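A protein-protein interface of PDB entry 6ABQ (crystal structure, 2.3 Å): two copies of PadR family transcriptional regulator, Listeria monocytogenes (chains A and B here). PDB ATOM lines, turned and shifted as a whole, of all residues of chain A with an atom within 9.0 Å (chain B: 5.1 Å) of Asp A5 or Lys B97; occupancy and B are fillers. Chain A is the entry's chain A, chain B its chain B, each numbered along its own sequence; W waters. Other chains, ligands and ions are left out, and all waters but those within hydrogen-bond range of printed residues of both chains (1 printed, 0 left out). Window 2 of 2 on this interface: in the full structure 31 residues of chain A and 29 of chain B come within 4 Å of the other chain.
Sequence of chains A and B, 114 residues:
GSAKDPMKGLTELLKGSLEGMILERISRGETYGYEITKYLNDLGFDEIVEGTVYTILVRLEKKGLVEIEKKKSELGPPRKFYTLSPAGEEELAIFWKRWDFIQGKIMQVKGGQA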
ATOM      1  N   SER A   2      -6.967 -31.256  24.825  1.00  0.00           N
ATOM      2  CA  SER A   2      -5.603 -31.763  24.979  1.00  0.00           C
ATOM      3  C   SER A   2      -5.092 -31.597  26.417  1.00  0.00           C
ATOM      4  O   SER A   2      -5.409 -30.605  27.088  1.00  0.00           O
ATOM      5  CB  SER A   2      -4.668 -31.049  24.001  1.00  0.00           C
ATOM      6  OG  SER A   2      -3.349 -31.563  24.075  1.00  0.00           O
ATOM      7  N   ALA A   3      -4.305 -32.574  26.873  1.00  0.00           N
ATOM      8  CA  ALA A   3      -3.691 -32.545  28.203  1.00  0.00           C
ATOM      9  C   ALA A   3      -2.755 -31.350  28.357  1.00  0.00           C
ATOM     10  O   ALA A   3      -2.045 -30.978  27.408  1.00  0.00           O
ATOM     11  CB  ALA A   3      -2.948 -33.841  28.479  1.00  0.00           C
ATOM     12  N   LYS A   4      -2.780 -30.747  29.547  1.00  0.00           N
ATOM     13  CA  LYS A   4      -1.937 -29.595  29.876  1.00  0.00           C
ATOM     14  C   LYS A   4      -0.468 -30.038  29.979  1.00  0.00           C
ATOM     15  O   LYS A   4      -0.104 -30.833  30.852  1.00  0.00           O
ATOM     16  CB  LYS A   4      -2.430 -28.908  31.166  1.00  0.00           C
ATOM     17  CG  LYS A   4      -2.195 -27.401  31.235  1.00  0.00           C
ATOM     18  CD  LYS A   4      -0.829 -27.057  31.810  1.00  0.00           C
ATOM     19  CE  LYS A   4      -0.399 -25.647  31.438  1.00  0.00           C
ATOM     20  NZ  LYS A   4       1.064 -25.473  31.650  1.00  0.00           N
ATOM     21  N   ASP A   5       0.349 -29.527  29.057  1.00  0.00           N
ATOM     22  CA  ASP A   5       1.756 -29.903  28.919  1.00  0.00           C
ATOM     23  C   ASP A   5       2.642 -28.996  29.789  1.00  0.00           C
ATOM     24  O   ASP A   5       2.707 -27.782  29.537  1.00  0.00           O
ATOM     25  CB  ASP A   5       2.167 -29.820  27.435  1.00  0.00           C
ATOM     26  CG  ASP A   5       3.482 -30.541  27.124  1.00  0.00           C
ATOM     27  OD1 ASP A   5       4.357 -30.672  28.008  1.00  0.00           O
ATOM     28  OD2 ASP A   5       3.646 -30.968  25.961  1.00  0.00           O
ATOM     29  N   PRO A   6       3.332 -29.577  30.811  1.00  0.00           N
ATOM     30  CA  PRO A   6       4.238 -28.812  31.688  1.00  0.00           C
ATOM     31  C   PRO A   6       5.531 -28.354  30.991  1.00  0.00           C
ATOM     32  O   PRO A   6       6.349 -27.668  31.607  1.00  0.00           O
ATOM     33  CB  PRO A   6       4.555 -29.805  32.814  1.00  0.00           C
ATOM     34  CG  PRO A   6       4.413 -31.143  32.173  1.00  0.00           C
ATOM     35  CD  PRO A   6       3.260 -30.993  31.227  1.00  0.00           C
ATOM     36  N   MET A   7       5.685 -28.747  29.724  1.00  0.00           N
ATOM     37  CA  MET A   7       6.798 -28.361  28.841  1.00  0.00           C
ATOM     38  C   MET A   7       8.163 -28.910  29.256  1.00  0.00           C
ATOM     39  O   MET A   7       9.070 -28.160  29.640  1.00  0.00           O
ATOM     40  CB  MET A   7       6.822 -26.842  28.573  1.00  0.00           C
ATOM     41  CG  MET A   7       6.602 -26.473  27.116  1.00  0.00           C
ATOM     42  SD  MET A   7       5.114 -27.133  26.339  1.00  0.00           S
ATOM     43  CE  MET A   7       5.732 -27.313  24.680  1.00  0.00           C
ATOM     44  N   LYS A   8       8.270 -30.236  29.188  1.00  0.00           N
ATOM     45  CA  LYS A   8       9.534 -30.954  29.327  1.00  0.00           C
ATOM     46  C   LYS A   8      10.072 -31.289  27.923  1.00  0.00           C
ATOM     47  O   LYS A   8       9.490 -30.870  26.910  1.00  0.00           O
ATOM     48  CB  LYS A   8       9.360 -32.240  30.164  1.00  0.00           C
ATOM     49  CG  LYS A   8       8.705 -32.087  31.537  1.00  0.00           C
ATOM     50  CD  LYS A   8       9.614 -31.402  32.542  1.00  0.00           C
ATOM     51  CE  LYS A   8       9.013 -31.425  33.934  1.00  0.00           C
ATOM     52  NZ  LYS A   8       9.816 -30.577  34.854  1.00  0.00           N
ATOM     53  N   GLY A   9      11.180 -32.031  27.875  1.00  0.00           N
ATOM     54  CA  GLY A   9      11.785 -32.480  26.618  1.00  0.00           C
ATOM     55  C   GLY A   9      12.383 -31.372  25.771  1.00  0.00           C
ATOM     56  O   GLY A   9      12.384 -31.467  24.546  1.00  0.00           O
ATOM     57  N   LEU A  10      12.898 -30.331  26.431  1.00  0.00           N
ATOM     58  CA  LEU A  10      13.462 -29.156  25.751  1.00  0.00           C
ATOM     59  C   LEU A  10      14.982 -29.197  25.556  1.00  0.00           C
ATOM     60  O   LEU A  10      15.539 -28.310  24.899  1.00  0.00           O
ATOM     61  CB  LEU A  10      13.077 -27.862  26.488  1.00  0.00           C
ATOM     62  CG  LEU A  10      11.622 -27.539  26.849  1.00  0.00           C
ATOM     63  CD1 LEU A  10      11.571 -26.325  27.764  1.00  0.00           C
ATOM     64  CD2 LEU A  10      10.757 -27.323  25.616  1.00  0.00           C
ATOM     65  N   LEU A  13      16.580 -28.996  21.854  1.00  0.00           N
ATOM     66  CA  LEU A  13      16.214 -27.702  21.254  1.00  0.00           C
ATOM     67  C   LEU A  13      16.940 -26.494  21.834  1.00  0.00           C
ATOM     68  O   LEU A  13      17.066 -25.472  21.160  1.00  0.00           O
ATOM     69  CB  LEU A  13      14.701 -27.471  21.350  1.00  0.00           C
ATOM     70  CG  LEU A  13      13.825 -27.734  20.125  1.00  0.00           C
ATOM     71  CD1 LEU A  13      13.737 -29.216  19.791  1.00  0.00           C
ATOM     72  CD2 LEU A  13      12.436 -27.144  20.322  1.00  0.00           C
ATOM     73  N   ASP A  46      13.125 -26.339  32.960  1.00  0.00           N
ATOM     74  CA  ASP A  46      13.027 -27.149  34.180  1.00  0.00           C
ATOM     75  C   ASP A  46      13.971 -28.334  34.297  1.00  0.00           C
ATOM     76  O   ASP A  46      14.181 -28.837  35.398  1.00  0.00           O
ATOM     77  CB  ASP A  46      11.598 -27.695  34.319  1.00  0.00           C
ATOM     78  CG  ASP A  46      10.736 -26.861  35.235  1.00  0.00           C
ATOM     79  OD1 ASP A  46      11.228 -26.439  36.311  1.00  0.00           O
ATOM     80  OD2 ASP A  46       9.553 -26.643  34.891  1.00  0.00           O
ATOM     81  N   LYS A 110       8.208 -22.163   9.103  1.00  0.00           N
ATOM     82  CA  LYS A 110       6.837 -22.316   9.610  1.00  0.00           C
ATOM     83  C   LYS A 110       5.759 -21.770   8.652  1.00  0.00           C
ATOM     84  O   LYS A 110       4.659 -22.326   8.574  1.00  0.00           O
ATOM     85  CB  LYS A 110       6.710 -21.646  10.982  1.00  0.00           C
ATOM     86  CG  LYS A 110       5.598 -22.206  11.853  1.00  0.00           C
ATOM     87  CD  LYS A 110       5.552 -21.522  13.207  1.00  0.00           C
ATOM     88  CE  LYS A 110       4.416 -22.067  14.054  1.00  0.00           C
ATOM     89  NZ  LYS A 110       4.286 -21.316  15.334  1.00  0.00           N
ATOM     90  N   ALA B  93       4.657 -31.600  15.324  1.00  0.00           N
ATOM     91  CA  ALA B  93       3.681 -30.837  16.120  1.00  0.00           C
ATOM     92  C   ALA B  93       4.249 -30.481  17.501  1.00  0.00           C
ATOM     93  O   ALA B  93       4.194 -29.319  17.923  1.00  0.00           O
ATOM     94  CB  ALA B  93       2.377 -31.613  16.255  1.00  0.00           C
ATOM     95  N   ILE B  94       4.810 -31.488  18.175  1.00  0.00           N
ATOM     96  CA  ILE B  94       5.527 -31.320  19.447  1.00  0.00           C
ATOM     97  C   ILE B  94       6.673 -30.297  19.294  1.00  0.00           C
ATOM     98  O   ILE B  94       6.821 -29.397  20.138  1.00  0.00           O
ATOM     99  CB  ILE B  94       6.053 -32.683  19.975  1.00  0.00           C
ATOM    100  CG1 ILE B  94       4.897 -33.556  20.477  1.00  0.00           C
ATOM    101  CG2 ILE B  94       7.098 -32.490  21.068  1.00  0.00           C
ATOM    102  CD1 ILE B  94       5.209 -35.039  20.504  1.00  0.00           C
ATOM    103  N   PHE B  95       7.449 -30.422  18.213  1.00  0.00           N
ATOM    104  CA  PHE B  95       8.533 -29.478  17.927  1.00  0.00           C
ATOM    105  C   PHE B  95       8.065 -28.017  17.888  1.00  0.00           C
ATOM    106  O   PHE B  95       8.695 -27.155  18.503  1.00  0.00           O
ATOM    107  CB  PHE B  95       9.298 -29.822  16.633  1.00  0.00           C
ATOM    108  CG  PHE B  95      10.193 -28.707  16.161  1.00  0.00           C
ATOM    109  CD1 PHE B  95      11.442 -28.502  16.755  1.00  0.00           C
ATOM    110  CD2 PHE B  95       9.766 -27.822  15.166  1.00  0.00           C
ATOM    111  CE1 PHE B  95      12.260 -27.455  16.344  1.00  0.00           C
ATOM    112  CE2 PHE B  95      10.578 -26.769  14.762  1.00  0.00           C
ATOM    113  CZ  PHE B  95      11.827 -26.588  15.347  1.00  0.00           C
ATOM    114  N   TRP B  96       6.984 -27.751  17.149  1.00  0.00           N
ATOM    115  CA  TRP B  96       6.455 -26.389  17.021  1.00  0.00           C
ATOM    116  C   TRP B  96       5.967 -25.820  18.343  1.00  0.00           C
ATOM    117  O   TRP B  96       6.247 -24.665  18.643  1.00  0.00           O
ATOM    118  CB  TRP B  96       5.403 -26.273  15.910  1.00  0.00           C
ATOM    119  CG  TRP B  96       6.038 -26.283  14.544  1.00  0.00           C
ATOM    120  CD1 TRP B  96       5.801 -27.173  13.537  1.00  0.00           C
ATOM    121  CD2 TRP B  96       7.050 -25.384  14.055  1.00  0.00           C
ATOM    122  NE1 TRP B  96       6.581 -26.872  12.445  1.00  0.00           N
ATOM    123  CE2 TRP B  96       7.362 -25.785  12.735  1.00  0.00           C
ATOM    124  CE3 TRP B  96       7.719 -24.271  14.604  1.00  0.00           C
ATOM    125  CZ2 TRP B  96       8.316 -25.121  11.948  1.00  0.00           C
ATOM    126  CZ3 TRP B  96       8.662 -23.608  13.822  1.00  0.00           C
ATOM    127  CH2 TRP B  96       8.955 -24.041  12.505  1.00  0.00           C
ATOM    128  N   LYS B  97       5.286 -26.652  19.133  1.00  0.00           N
ATOM    129  CA  LYS B  97       4.843 -26.295  20.482  1.00  0.00           C
ATOM    130  C   LYS B  97       6.029 -25.975  21.407  1.00  0.00           C
ATOM    131  O   LYS B  97       6.020 -24.942  22.082  1.00  0.00           O
ATOM    132  CB  LYS B  97       3.958 -27.399  21.081  1.00  0.00           C
ATOM    133  CG  LYS B  97       3.087 -26.917  22.229  1.00  0.00           C
ATOM    134  CD  LYS B  97       2.206 -28.007  22.823  1.00  0.00           C
ATOM    135  CE  LYS B  97       1.556 -27.496  24.101  1.00  0.00           C
ATOM    136  NZ  LYS B  97       0.454 -28.372  24.594  1.00  0.00           N
ATOM    137  N   ARG B  98       7.035 -26.857  21.421  1.00  0.00           N
ATOM    138  CA  ARG B  98       8.265 -26.665  22.216  1.00  0.00           C
ATOM    139  C   ARG B  98       9.058 -25.428  21.785  1.00  0.00           C
ATOM    140  O   ARG B  98       9.523 -24.665  22.641  1.00  0.00           O
ATOM    141  CB  ARG B  98       9.169 -27.910  22.172  1.00  0.00           C
ATOM    142  CG  ARG B  98       8.654 -29.116  22.937  1.00  0.00           C
ATOM    143  CD  ARG B  98       9.633 -30.274  22.847  1.00  0.00           C
ATOM    144  NE  ARG B  98       9.208 -31.416  23.655  1.00  0.00           N
ATOM    145  CZ  ARG B  98       9.558 -32.688  23.440  1.00  0.00           C
ATOM    146  NH1 ARG B  98      10.336 -33.023  22.411  1.00  0.00           N
ATOM    147  NH2 ARG B  98       9.100 -33.639  24.251  1.00  0.00           N
ATOM    148  N   TRP B  99       9.196 -25.239  20.468  1.00  0.00           N
ATOM    149  CA  TRP B  99       9.926 -24.094  19.911  1.00  0.00           C
ATOM    150  C   TRP B  99       9.250 -22.747  20.214  1.00  0.00           C
ATOM    151  O   TRP B  99       9.942 -21.766  20.485  1.00  0.00           O
ATOM    152  CB  TRP B  99      10.175 -24.249  18.405  1.00  0.00           C
ATOM    153  CG  TRP B  99      10.995 -23.125  17.843  1.00  0.00           C
ATOM    154  CD1 TRP B  99      12.356 -22.985  17.913  1.00  0.00           C
ATOM    155  CD2 TRP B  99      10.506 -21.961  17.165  1.00  0.00           C
ATOM    156  NE1 TRP B  99      12.745 -21.815  17.305  1.00  0.00           N
ATOM    157  CE2 TRP B  99      11.632 -21.164  16.839  1.00  0.00           C
ATOM    158  CE3 TRP B  99       9.225 -21.517  16.792  1.00  0.00           C
ATOM    159  CZ2 TRP B  99      11.519 -19.942  16.153  1.00  0.00           C
ATOM    160  CZ3 TRP B  99       9.109 -20.304  16.109  1.00  0.00           C
ATOM    161  CH2 TRP B  99      10.258 -19.532  15.794  1.00  0.00           C
ATOM    162  N   ASP B 100       7.915 -22.713  20.161  1.00  0.00           N
ATOM    163  CA  ASP B 100       7.157 -21.500  20.507  1.00  0.00           C
ATOM    164  C   ASP B 100       7.284 -21.124  21.988  1.00  0.00           C
ATOM    165  O   ASP B 100       7.435 -19.953  22.311  1.00  0.00           O
ATOM    166  CB  ASP B 100       5.691 -21.603  20.073  1.00  0.00           C
ATOM    167  CG  ASP B 100       5.507 -21.381  18.577  1.00  0.00           C
ATOM    168  OD1 ASP B 100       6.061 -20.398  18.018  1.00  0.00           O
ATOM    169  OD2 ASP B 100       4.787 -22.183  17.953  1.00  0.00           O
ATOM    170  N   PHE B 101       7.244 -22.121  22.871  1.00  0.00           N
ATOM    171  CA  PHE B 101       7.497 -21.921  24.303  1.00  0.00           C
ATOM    172  C   PHE B 101       8.901 -21.341  24.554  1.00  0.00           C
ATOM    173  O   PHE B 101       9.035 -20.349  25.269  1.00  0.00           O
ATOM    174  CB  PHE B 101       7.263 -23.224  25.096  1.00  0.00           C
ATOM    175  CG  PHE B 101       7.602 -23.117  26.566  1.00  0.00           C
ATOM    176  CD1 PHE B 101       6.647 -22.684  27.491  1.00  0.00           C
ATOM    177  CD2 PHE B 101       8.883 -23.460  27.035  1.00  0.00           C
ATOM    178  CE1 PHE B 101       6.960 -22.585  28.847  1.00  0.00           C
ATOM    179  CE2 PHE B 101       9.201 -23.361  28.389  1.00  0.00           C
ATOM    180  CZ  PHE B 101       8.238 -22.922  29.298  1.00  0.00           C
HETATM  181  O   HOH W   1       7.778 -33.891  26.586  1.00  0.00           O
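The backbone NH (N) of Met A7 lies within hydrogen-bond range of the side-chain carboxylate (OD1) of Asp A5 (2.9 Å). NZ of Lys A8 lies within salt-bridge range of OD2 of Asp A46, at 3.9 Å.
Of the 9 printed residues of chain B, 7 touch a printed residue of chain A. Printed residues of chain B that touch a printed residue of chain A: Phe B95, Trp B96, Lys B97, Arg B98, Trp B99, Asp B100 and Phe B101. Hydrophobic or aromatic side chains of chain B that line the printed part of chain A: Phe B95, Trp B96 and Phe B101. Printed residues of chain A that touch a printed residue of chain B: Asp A5, Met A7, Lys A8, Gly A9, Leu A10, Leu A13 and Lys A110. Hydrophobic or aromatic side chains of chain A within 4 Å of the printed part of chain B: Met A7, Leu A10 and Leu A13. Along chain A the printed residues that touch a printed residue of chain B span positions 5 to 110. Among the printed residues, Asp or Glu carboxylates within 4 Å of a Lys or Arg side-chain nitrogen of the other chain: Lys A110 with Asp B100.
CB of Asp A5 touches NZ of Lys B97 (3.6 Å). CE of Met A7 touches O of Lys B97, at 3.5 Å. CE of Met A7 touches N of Arg B98, at 3.5 Å. Met A7 touches Phe B101 (CG to CG, 3.5 Å). CD2 of Leu A10 touches CB of Arg B98 (3.8 Å). Leu A10 touches Phe B101. Phe B95 touches Leu A13 (CD1 to CD1, 3.9 Å). CD2 of Leu A13 touches CB of Arg B98 (3.8 Å). Leu A13 touches Trp B99 (CD2 to N, 3.8 Å). CH2 of Trp B96 touches CB of Lys A110, at 3.6 Å.
Asp A5 touches just one residue of chain B: Lys B97 (3.6 Å). Of chain A, only Asp A5 and Met A7 come within 4 Å of Lys B97. Of the printed residues of chain A, Trp B96 touches Lys A110. Of the printed residues of chain A, Asp B100 touches Lys A110 (2.8 Å). Ala A3 touches none of the printed residues of chain B. The nearest residue of chain A that does not touch Lys B97 is Ala A3 (4.6 Å). The nearest printed residue of chain B that does not touch Lys A110 is Trp B99 (4.7 Å).
No position is printed for both chains. Of the 13 pairs that touch across the chains among the printed residues, none has its exchanged pair printed and touching as well.
The guanidinium group (NE) of Arg B98 lies within hydrogen-bond range of the backbone carbonyl oxygen (O) of Lys A8 (3.3 Å). The guanidinium group (NE) of Arg B98 lies close to the backbone carbonyl oxygen (O) of Gly A9. NZ of Lys A110 is in salt-bridge range of OD2 of Asp B100 (2.8 Å).
Water W1 lies within hydrogen-bond range of NH2 of Arg B98 (2.7 Å) and O of Lys A8 (3.5 Å).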
